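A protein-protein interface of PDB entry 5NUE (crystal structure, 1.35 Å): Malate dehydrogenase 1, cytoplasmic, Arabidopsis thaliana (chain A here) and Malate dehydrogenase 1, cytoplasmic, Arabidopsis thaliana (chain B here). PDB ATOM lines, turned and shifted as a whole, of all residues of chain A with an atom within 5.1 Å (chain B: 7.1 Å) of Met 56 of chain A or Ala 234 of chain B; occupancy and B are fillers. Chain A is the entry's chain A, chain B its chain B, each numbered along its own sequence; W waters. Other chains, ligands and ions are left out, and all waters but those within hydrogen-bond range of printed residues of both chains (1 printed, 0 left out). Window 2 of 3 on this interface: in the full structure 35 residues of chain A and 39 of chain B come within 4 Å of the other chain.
Of the 9 printed residues of chain A, 4 touch a printed residue of chain B. Hydrophobic or aromatic side chains of chain A within 4 Å of the printed part of chain B: Met 56. Of the 18 printed residues of chain B, 8 touch a printed residue of chain A. Printed residues of chain B that touch a printed residue of chain A: Arg 163, Arg 231, Ala 234, Ile 235, Ala 238, Arg 239, Ser 243 and Ser 246. Hydrophobic or aromatic side chains of chain B within 4 Å of the printed part of chain A: Ala 234, Ile 235 and Ala 238. Among the printed residues, Asp or Glu carboxylates within 4 Å of a Lys or Arg side-chain nitrogen of the other chain: Glu 57 of chain A with Arg 239 of chain B (3.1 Å), Asp 60 of chain A with Arg 163 of chain B (3.9 Å) and Asp 60 of chain A with Arg 231 of chain B (2.8 Å).
The side-chain carboxylate (OE1) of Glu 57 of chain A lies within hydrogen-bond range of the side-chain hydroxyl (OG) of Ser 246 of chain B (2.8 Å). The side-chain carboxylate of Glu 57 of chain A is in salt-bridge range of the guanidinium group of Arg 239 of chain B, 3.1 Å away. The side-chain carboxylate (OD2) of Asp 60 of chain A lies within salt-bridge range of the guanidinium group (NE) of Arg 163 of chain B, 3.9 Å away. O of Ser 243 of chain B lies close to OE1 of Glu 57 of chain A (3.2 Å). The backbone carbonyl oxygen of Met 56 of chain A lies within hydrogen-bond range of the guanidinium group of Arg 231 of chain B (3.1 Å). The guanidinium group (NH2) of Arg 231 of chain B is in salt-bridge range of the side-chain carboxylate (OD1) of Asp 60 of chain A (2.8 Å).
Of the printed residues of chain A, Ala 234 of chain B touches Met 56 (3.8 Å). Printed residues of chain B within 4 Å of Glu 57 of chain A: Ile 235, Arg 239, Ser 243 and Ser 246. Of the printed residues of chain A, Arg 163 of chain B touches Asp 60. Lys 55 of chain A touches none of the printed residues of chain B. Thr 227 of chain B touches none of the printed residues of chain A. The nearest printed residue of chain A that does not touch Ala 234 of chain B is Gly 53 of chain A (6.2 Å). The nearest printed residue of chain B that does not touch Gly 53 of chain A is Ile 235 of chain B (4.1 Å).
The guanidinium group of Arg 163 of chain B sits at hydrogen-bond distance from the side-chain hydroxyl of Ser 243 of chain B, 3.0 Å away. The guanidinium group of Arg 239 of chain B is in hydrogen-bond range of the backbone carbonyl oxygen of Leu 241 of chain B (3.4 Å). OD1 of Asn 52 of chain A sits close to SD of Met 56 of chain A (3.5 Å). The backbone carbonyl oxygen of Ser 243 of chain B lies close to the side-chain hydroxyl of Ser 246 of chain B (3.4 Å).
Ala 238 of chain B touches Gly 53 of chain A. CE of Met 56 of chain A touches CB of Ala 234 of chain B, at 3.8 Å. CD1 of Ile 235 of chain B touches CB of Met 56 of chain A, at 3.6 Å. Glu 57 of chain A touches Ile 235 of chain B. Asp 60 of chain A touches Ile 235 of chain B.
Water W1 lies within hydrogen-bond range of OD2 of Asp 60 of chain A (2.7 Å), OG of Ser 246 of chain B (2.9 Å), NE of Arg 163 of chain B (3.0 Å) and OG of Ser 243 of chain B (3.4 Å).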
ATOM      1  N   ASN A  52      15.125 -25.175 -14.789  1.00  0.00           N
ATOM      2  CA  ASN A  52      15.844 -24.925 -16.026  1.00  0.00           C
ATOM      3  C   ASN A  52      17.348 -25.003 -15.796  1.00  0.00           C
ATOM      4  O   ASN A  52      18.102 -25.465 -16.676  1.00  0.00           O
ATOM      5  CB  ASN A  52      15.451 -23.556 -16.572  1.00  0.00           C
ATOM      6  CG  ASN A  52      16.141 -23.255 -17.872  1.00  0.00           C
ATOM      7  OD1 ASN A  52      16.976 -22.340 -17.969  1.00  0.00           O
ATOM      8  ND2 ASN A  52      15.848 -24.063 -18.881  1.00  0.00           N
ATOM      9  N   GLY A  53      17.808 -24.540 -14.625  1.00  0.00           N
ATOM     10  CA  GLY A  53      19.223 -24.695 -14.284  1.00  0.00           C
ATOM     11  C   GLY A  53      19.668 -26.149 -14.212  1.00  0.00           C
ATOM     12  O   GLY A  53      20.797 -26.479 -14.603  1.00  0.00           O
ATOM     13  N   VAL A  54      18.814 -27.031 -13.682  1.00  0.00           N
ATOM     14  CA  VAL A  54      19.162 -28.455 -13.641  1.00  0.00           C
ATOM     15  C   VAL A  54      19.319 -29.003 -15.050  1.00  0.00           C
ATOM     16  O   VAL A  54      20.288 -29.713 -15.346  1.00  0.00           O
ATOM     17  CB  VAL A  54      18.117 -29.262 -12.863  1.00  0.00           C
ATOM     18  CG1 VAL A  54      18.474 -30.778 -12.865  1.00  0.00           C
ATOM     19  CG2 VAL A  54      18.006 -28.739 -11.419  1.00  0.00           C
ATOM     20  N   LYS A  55      18.395 -28.663 -15.947  1.00  0.00           N
ATOM     21  CA  LYS A  55      18.537 -29.090 -17.336  1.00  0.00           C
ATOM     22  C   LYS A  55      19.834 -28.571 -17.943  1.00  0.00           C
ATOM     23  O   LYS A  55      20.543 -29.321 -18.646  1.00  0.00           O
ATOM     24  CB  LYS A  55      17.327 -28.630 -18.169  1.00  0.00           C
ATOM     25  CG  LYS A  55      17.506 -28.927 -19.680  1.00  0.00           C
ATOM     26  CD  LYS A  55      16.226 -28.772 -20.488  1.00  0.00           C
ATOM     27  CE  LYS A  55      16.532 -28.983 -21.997  1.00  0.00           C
ATOM     28  NZ  LYS A  55      15.290 -29.051 -22.828  1.00  0.00           N
ATOM     29  N   MET A  56      20.169 -27.299 -17.686  1.00  0.00           N
ATOM     30  CA  MET A  56      21.417 -26.716 -18.209  1.00  0.00           C
ATOM     31  C   MET A  56      22.633 -27.508 -17.733  1.00  0.00           C
ATOM     32  O   MET A  56      23.605 -27.662 -18.482  1.00  0.00           O
ATOM     33  CB  MET A  56      21.606 -25.255 -17.833  1.00  0.00           C
ATOM     34  CG  MET A  56      20.629 -24.302 -18.557  1.00  0.00           C
ATOM     35  SD  MET A  56      20.440 -22.777 -17.644  1.00  0.00           S
ATOM     36  CE  MET A  56      21.924 -21.898 -18.157  1.00  0.00           C
ATOM     37  N   GLU A  57      22.626 -27.951 -16.464  1.00  0.00           N
ATOM     38  CA  GLU A  57      23.754 -28.728 -15.956  1.00  0.00           C
ATOM     39  C   GLU A  57      23.795 -30.141 -16.524  1.00  0.00           C
ATOM     40  O   GLU A  57      24.896 -30.704 -16.690  1.00  0.00           O
ATOM     41  CB  GLU A  57      23.735 -28.797 -14.427  1.00  0.00           C
ATOM     42  CG  GLU A  57      24.132 -27.493 -13.737  1.00  0.00           C
ATOM     43  CD  GLU A  57      24.652 -27.779 -12.329  1.00  0.00           C
ATOM     44  OE1 GLU A  57      25.761 -28.374 -12.184  1.00  0.00           O
ATOM     45  OE2 GLU A  57      23.950 -27.409 -11.349  1.00  0.00           O
ATOM     46  N   LEU A  58      22.637 -30.757 -16.762  1.00  0.00           N
ATOM     47  CA  LEU A  58      22.609 -32.085 -17.367  1.00  0.00           C
ATOM     48  C   LEU A  58      23.225 -32.026 -18.757  1.00  0.00           C
ATOM     49  O   LEU A  58      24.001 -32.909 -19.142  1.00  0.00           O
ATOM     50  CB  LEU A  58      21.165 -32.621 -17.468  1.00  0.00           C
ATOM     51  CG  LEU A  58      20.578 -33.114 -16.116  1.00  0.00           C
ATOM     52  CD1 LEU A  58      19.062 -33.319 -16.222  1.00  0.00           C
ATOM     53  CD2 LEU A  58      21.287 -34.388 -15.576  1.00  0.00           C
ATOM     54  N   ILE A  59      22.883 -30.994 -19.531  1.00  0.00           N
ATOM     55  CA  ILE A  59      23.535 -30.771 -20.830  1.00  0.00           C
ATOM     56  C   ILE A  59      25.040 -30.536 -20.667  1.00  0.00           C
ATOM     57  O   ILE A  59      25.859 -31.063 -21.449  1.00  0.00           O
ATOM     58  CB  ILE A  59      22.834 -29.606 -21.546  1.00  0.00           C
ATOM     59  CG1 ILE A  59      21.446 -30.045 -21.989  1.00  0.00           C
ATOM     60  CG2 ILE A  59      23.680 -29.117 -22.745  1.00  0.00           C
ATOM     61  CD1 ILE A  59      20.546 -28.850 -22.344  1.00  0.00           C
ATOM     62  N   ASP A  60      25.434 -29.729 -19.671  1.00  0.00           N
ATOM     63  CA  ASP A  60      26.833 -29.376 -19.469  1.00  0.00           C
ATOM     64  C   ASP A  60      27.691 -30.559 -19.086  1.00  0.00           C
ATOM     65  O   ASP A  60      28.901 -30.513 -19.304  1.00  0.00           O
ATOM     66  CB  ASP A  60      26.950 -28.300 -18.389  1.00  0.00           C
ATOM     67  CG  ASP A  60      26.354 -26.970 -18.829  1.00  0.00           C
ATOM     68  OD1 ASP A  60      26.036 -26.800 -20.032  1.00  0.00           O
ATOM     69  OD2 ASP A  60      26.208 -26.078 -17.966  1.00  0.00           O
ATOM     70  N   ARG B  93      32.139 -18.648  -5.735  1.00  0.00           N
ATOM     71  CA  ARG B  93      31.817 -17.251  -5.978  1.00  0.00           C
ATOM     72  C   ARG B  93      30.309 -17.036  -5.872  1.00  0.00           C
ATOM     73  O   ARG B  93      29.504 -17.963  -6.018  1.00  0.00           O
ATOM     74  CB  ARG B  93      32.369 -16.737  -7.312  1.00  0.00           C
ATOM     75  CG  ARG B  93      32.001 -17.567  -8.497  1.00  0.00           C
ATOM     76  CD  ARG B  93      32.218 -16.855  -9.836  1.00  0.00           C
ATOM     77  NE  ARG B  93      31.946 -17.812 -10.880  1.00  0.00           N
ATOM     78  CZ  ARG B  93      31.755 -17.507 -12.164  1.00  0.00           C
ATOM     79  NH1 ARG B  93      31.745 -16.231 -12.565  1.00  0.00           N
ATOM     80  NH2 ARG B  93      31.563 -18.482 -13.045  1.00  0.00           N
ATOM     81  N   ARG B 163      30.880 -28.604 -21.296  1.00  0.00           N
ATOM     82  CA  ARG B 163      29.920 -27.556 -21.672  1.00  0.00           C
ATOM     83  C   ARG B 163      29.976 -27.288 -23.166  1.00  0.00           C
ATOM     84  O   ARG B 163      28.924 -27.079 -23.817  1.00  0.00           O
ATOM     85  CB  ARG B 163      30.240 -26.261 -20.920  1.00  0.00           C
ATOM     86  CG  ARG B 163      29.773 -26.297 -19.427  1.00  0.00           C
ATOM     87  CD  ARG B 163      30.483 -25.225 -18.630  1.00  0.00           C
ATOM     88  NE  ARG B 163      29.877 -25.086 -17.286  1.00  0.00           N
ATOM     89  CZ  ARG B 163      30.452 -24.429 -16.280  1.00  0.00           C
ATOM     90  NH1 ARG B 163      31.640 -23.856 -16.456  1.00  0.00           N
ATOM     91  NH2 ARG B 163      29.826 -24.321 -15.080  1.00  0.00           N
ATOM     92  N   GLN B 167      27.005 -27.706 -25.851  1.00  0.00           N
ATOM     93  CA  GLN B 167      26.510 -26.650 -26.753  1.00  0.00           C
ATOM     94  C   GLN B 167      26.445 -27.127 -28.200  1.00  0.00           C
ATOM     95  O   GLN B 167      25.527 -26.755 -28.944  1.00  0.00           O
ATOM     96  CB  GLN B 167      27.401 -25.418 -26.688  1.00  0.00           C
ATOM     97  CG  GLN B 167      27.237 -24.622 -25.412  1.00  0.00           C
ATOM     98  CD  GLN B 167      25.844 -24.077 -25.318  1.00  0.00           C
ATOM     99  OE1 GLN B 167      25.392 -23.406 -26.237  1.00  0.00           O
ATOM    100  NE2 GLN B 167      25.183 -24.300 -24.206  1.00  0.00           N
ATOM    101  N   THR B 227      29.129 -18.063 -24.599  1.00  0.00           N
ATOM    102  CA  THR B 227      28.231 -18.948 -23.853  1.00  0.00           C
ATOM    103  C   THR B 227      29.013 -19.927 -22.978  1.00  0.00           C
ATOM    104  O   THR B 227      28.721 -20.095 -21.782  1.00  0.00           O
ATOM    105  CB  THR B 227      27.286 -19.676 -24.794  1.00  0.00           C
ATOM    106  OG1 THR B 227      26.356 -18.729 -25.340  1.00  0.00           O
ATOM    107  CG2 THR B 227      26.525 -20.735 -24.055  1.00  0.00           C
ATOM    108  N   GLN B 230      30.782 -18.036 -20.067  1.00  0.00           N
ATOM    109  CA  GLN B 230      29.898 -17.467 -19.056  1.00  0.00           C
ATOM    110  C   GLN B 230      28.935 -18.474 -18.458  1.00  0.00           C
ATOM    111  O   GLN B 230      28.033 -18.086 -17.701  1.00  0.00           O
ATOM    112  CB  GLN B 230      29.137 -16.263 -19.617  1.00  0.00           C
ATOM    113  CG  GLN B 230      30.057 -15.099 -19.985  1.00  0.00           C
ATOM    114  CD  GLN B 230      30.827 -14.588 -18.771  1.00  0.00           C
ATOM    115  OE1 GLN B 230      32.037 -14.293 -18.858  1.00  0.00           O
ATOM    116  NE2 GLN B 230      30.153 -14.508 -17.632  1.00  0.00           N
ATOM    117  N   ARG B 231      29.105 -19.757 -18.767  1.00  0.00           N
ATOM    118  CA  ARG B 231      28.114 -20.757 -18.382  1.00  0.00           C
ATOM    119  C   ARG B 231      28.002 -20.907 -16.865  1.00  0.00           C
ATOM    120  O   ARG B 231      26.893 -21.028 -16.334  1.00  0.00           O
ATOM    121  CB  ARG B 231      28.416 -22.090 -19.080  1.00  0.00           C
ATOM    122  CG  ARG B 231      27.373 -23.180 -18.876  1.00  0.00           C
ATOM    123  CD  ARG B 231      26.000 -22.777 -19.447  1.00  0.00           C
ATOM    124  NE  ARG B 231      25.258 -24.009 -19.650  1.00  0.00           N
ATOM    125  CZ  ARG B 231      24.220 -24.149 -20.453  1.00  0.00           C
ATOM    126  NH1 ARG B 231      23.733 -23.095 -21.121  1.00  0.00           N
ATOM    127  NH2 ARG B 231      23.684 -25.356 -20.594  1.00  0.00           N
ATOM    128  N   GLY B 232      29.133 -20.905 -16.151  1.00  0.00           N
ATOM    129  CA  GLY B 232      29.067 -20.992 -14.698  1.00  0.00           C
ATOM    130  C   GLY B 232      28.253 -19.868 -14.075  1.00  0.00           C
ATOM    131  O   GLY B 232      27.479 -20.094 -13.143  1.00  0.00           O
ATOM    132  N   ALA B 233      28.412 -18.639 -14.585  1.00  0.00           N
ATOM    133  CA  ALA B 233      27.616 -17.537 -14.063  1.00  0.00           C
ATOM    134  C   ALA B 233      26.138 -17.729 -14.384  1.00  0.00           C
ATOM    135  O   ALA B 233      25.275 -17.355 -13.575  1.00  0.00           O
ATOM    136  CB  ALA B 233      28.148 -16.215 -14.599  1.00  0.00           C
ATOM    137  N   ALA B 234      25.821 -18.313 -15.547  1.00  0.00           N
ATOM    138  CA  ALA B 234      24.425 -18.588 -15.889  1.00  0.00           C
ATOM    139  C   ALA B 234      23.809 -19.618 -14.938  1.00  0.00           C
ATOM    140  O   ALA B 234      22.638 -19.501 -14.554  1.00  0.00           O
ATOM    141  CB  ALA B 234      24.365 -19.097 -17.331  1.00  0.00           C
ATOM    142  N   ILE B 235      24.570 -20.642 -14.556  1.00  0.00           N
ATOM    143  CA  ILE B 235      24.046 -21.615 -13.596  1.00  0.00           C
ATOM    144  C   ILE B 235      23.758 -20.943 -12.272  1.00  0.00           C
ATOM    145  O   ILE B 235      22.725 -21.191 -11.651  1.00  0.00           O
ATOM    146  CB  ILE B 235      25.015 -22.788 -13.400  1.00  0.00           C
ATOM    147  CG1 ILE B 235      25.255 -23.503 -14.734  1.00  0.00           C
ATOM    148  CG2 ILE B 235      24.465 -23.746 -12.314  1.00  0.00           C
ATOM    149  CD1 ILE B 235      24.019 -24.072 -15.447  1.00  0.00           C
ATOM    150  N   ILE B 236      24.689 -20.120 -11.789  1.00  0.00           N
ATOM    151  CA  ILE B 236      24.480 -19.431 -10.509  1.00  0.00           C
ATOM    152  C   ILE B 236      23.239 -18.537 -10.578  1.00  0.00           C
ATOM    153  O   ILE B 236      22.495 -18.394  -9.587  1.00  0.00           O
ATOM    154  CB  ILE B 236      25.759 -18.659 -10.104  1.00  0.00           C
ATOM    155  CG1 ILE B 236      26.963 -19.613  -9.946  1.00  0.00           C
ATOM    156  CG2 ILE B 236      25.514 -17.803  -8.832  1.00  0.00           C
ATOM    157  CD1 ILE B 236      28.423 -19.004 -10.201  1.00  0.00           C
ATOM    158  N   LYS B 237      22.999 -17.911 -11.744  1.00  0.00           N
ATOM    159  CA  LYS B 237      21.828 -17.042 -11.902  1.00  0.00           C
ATOM    160  C   LYS B 237      20.554 -17.867 -11.789  1.00  0.00           C
ATOM    161  O   LYS B 237      19.572 -17.437 -11.166  1.00  0.00           O
ATOM    162  CB  LYS B 237      21.885 -16.343 -13.274  1.00  0.00           C
ATOM    163  CG  LYS B 237      20.839 -15.215 -13.508  1.00  0.00           C
ATOM    164  CD  LYS B 237      21.237 -13.958 -12.721  1.00  0.00           C
ATOM    165  CE  LYS B 237      20.311 -12.764 -12.915  1.00  0.00           C
ATOM    166  NZ  LYS B 237      20.161 -12.231 -14.307  1.00  0.00           N
ATOM    167  N   ALA B 238      20.566 -19.072 -12.367  1.00  0.00           N
ATOM    168  CA  ALA B 238      19.376 -19.916 -12.375  1.00  0.00           C
ATOM    169  C   ALA B 238      19.133 -20.553 -11.020  1.00  0.00           C
ATOM    170  O   ALA B 238      17.989 -20.619 -10.566  1.00  0.00           O
ATOM    171  CB  ALA B 238      19.521 -21.012 -13.430  1.00  0.00           C
ATOM    172  N   ARG B 239      20.201 -21.035 -10.364  1.00  0.00           N
ATOM    173  CA  ARG B 239      20.072 -21.871  -9.175  1.00  0.00           C
ATOM    174  C   ARG B 239      20.427 -21.181  -7.860  1.00  0.00           C
ATOM    175  O   ARG B 239      20.107 -21.728  -6.800  1.00  0.00           O
ATOM    176  CB  ARG B 239      20.941 -23.129  -9.316  1.00  0.00           C
ATOM    177  CG  ARG B 239      20.477 -24.044 -10.417  1.00  0.00           C
ATOM    178  CD  ARG B 239      21.337 -25.314 -10.379  1.00  0.00           C
ATOM    179  NE  ARG B 239      21.410 -25.871  -9.026  1.00  0.00           N
ATOM    180  CZ  ARG B 239      22.523 -25.951  -8.301  1.00  0.00           C
ATOM    181  NH1 ARG B 239      23.688 -25.585  -8.836  1.00  0.00           N
ATOM    182  NH2 ARG B 239      22.489 -26.452  -7.069  1.00  0.00           N
ATOM    183  N   LYS B 240      21.094 -20.025  -7.886  1.00  0.00           N
ATOM    184  CA  LYS B 240      21.625 -19.366  -6.692  1.00  0.00           C
ATOM    185  C   LYS B 240      22.720 -20.162  -6.003  1.00  0.00           C
ATOM    186  O   LYS B 240      23.105 -19.842  -4.871  1.00  0.00           O
ATOM    187  CB  LYS B 240      20.512 -18.964  -5.702  1.00  0.00           C
ATOM    188  CG  LYS B 240      19.291 -18.436  -6.427  1.00  0.00           C
ATOM    189  CD  LYS B 240      19.667 -17.250  -7.274  1.00  0.00           C
ATOM    190  CE  LYS B 240      18.459 -16.583  -7.932  1.00  0.00           C
ATOM    191  NZ  LYS B 240      18.891 -15.740  -9.106  1.00  0.00           N
ATOM    192  N   LEU B 241      23.239 -21.170  -6.668  1.00  0.00           N
ATOM    193  CA  LEU B 241      24.491 -21.787  -6.307  1.00  0.00           C
ATOM    194  C   LEU B 241      25.194 -22.079  -7.622  1.00  0.00           C
ATOM    195  O   LEU B 241      24.552 -22.328  -8.651  1.00  0.00           O
ATOM    196  CB  LEU B 241      24.257 -23.058  -5.498  1.00  0.00           C
ATOM    197  CG  LEU B 241      23.442 -22.721  -4.244  1.00  0.00           C
ATOM    198  CD1 LEU B 241      22.891 -23.960  -3.559  1.00  0.00           C
ATOM    199  CD2 LEU B 241      24.307 -21.939  -3.266  1.00  0.00           C
ATOM    200  N   SER B 243      27.513 -24.930 -10.085  1.00  0.00           N
ATOM    201  CA  SER B 243      27.293 -26.034 -11.021  1.00  0.00           C
ATOM    202  C   SER B 243      27.824 -27.347 -10.480  1.00  0.00           C
ATOM    203  O   SER B 243      28.758 -27.921 -11.026  1.00  0.00           O
ATOM    204  CB  SER B 243      28.043 -25.839 -12.344  1.00  0.00           C
ATOM    205  OG  SER B 243      27.810 -24.588 -12.854  1.00  0.00           O
ATOM    206  N   SER B 246      27.318 -30.897 -12.417  1.00  0.00           N
ATOM    207  CA  SER B 246      28.114 -31.006 -13.635  1.00  0.00           C
ATOM    208  C   SER B 246      29.595 -30.881 -13.311  1.00  0.00           C
ATOM    209  O   SER B 246      30.419 -31.481 -14.005  1.00  0.00           O
ATOM    210  CB  SER B 246      27.592 -29.989 -14.669  1.00  0.00           C
ATOM    211  OG  SER B 246      27.670 -28.677 -14.174  1.00  0.00           O
HETATM  212  O   HOH W   1      27.659 -26.285 -15.750  1.00  0.00           O
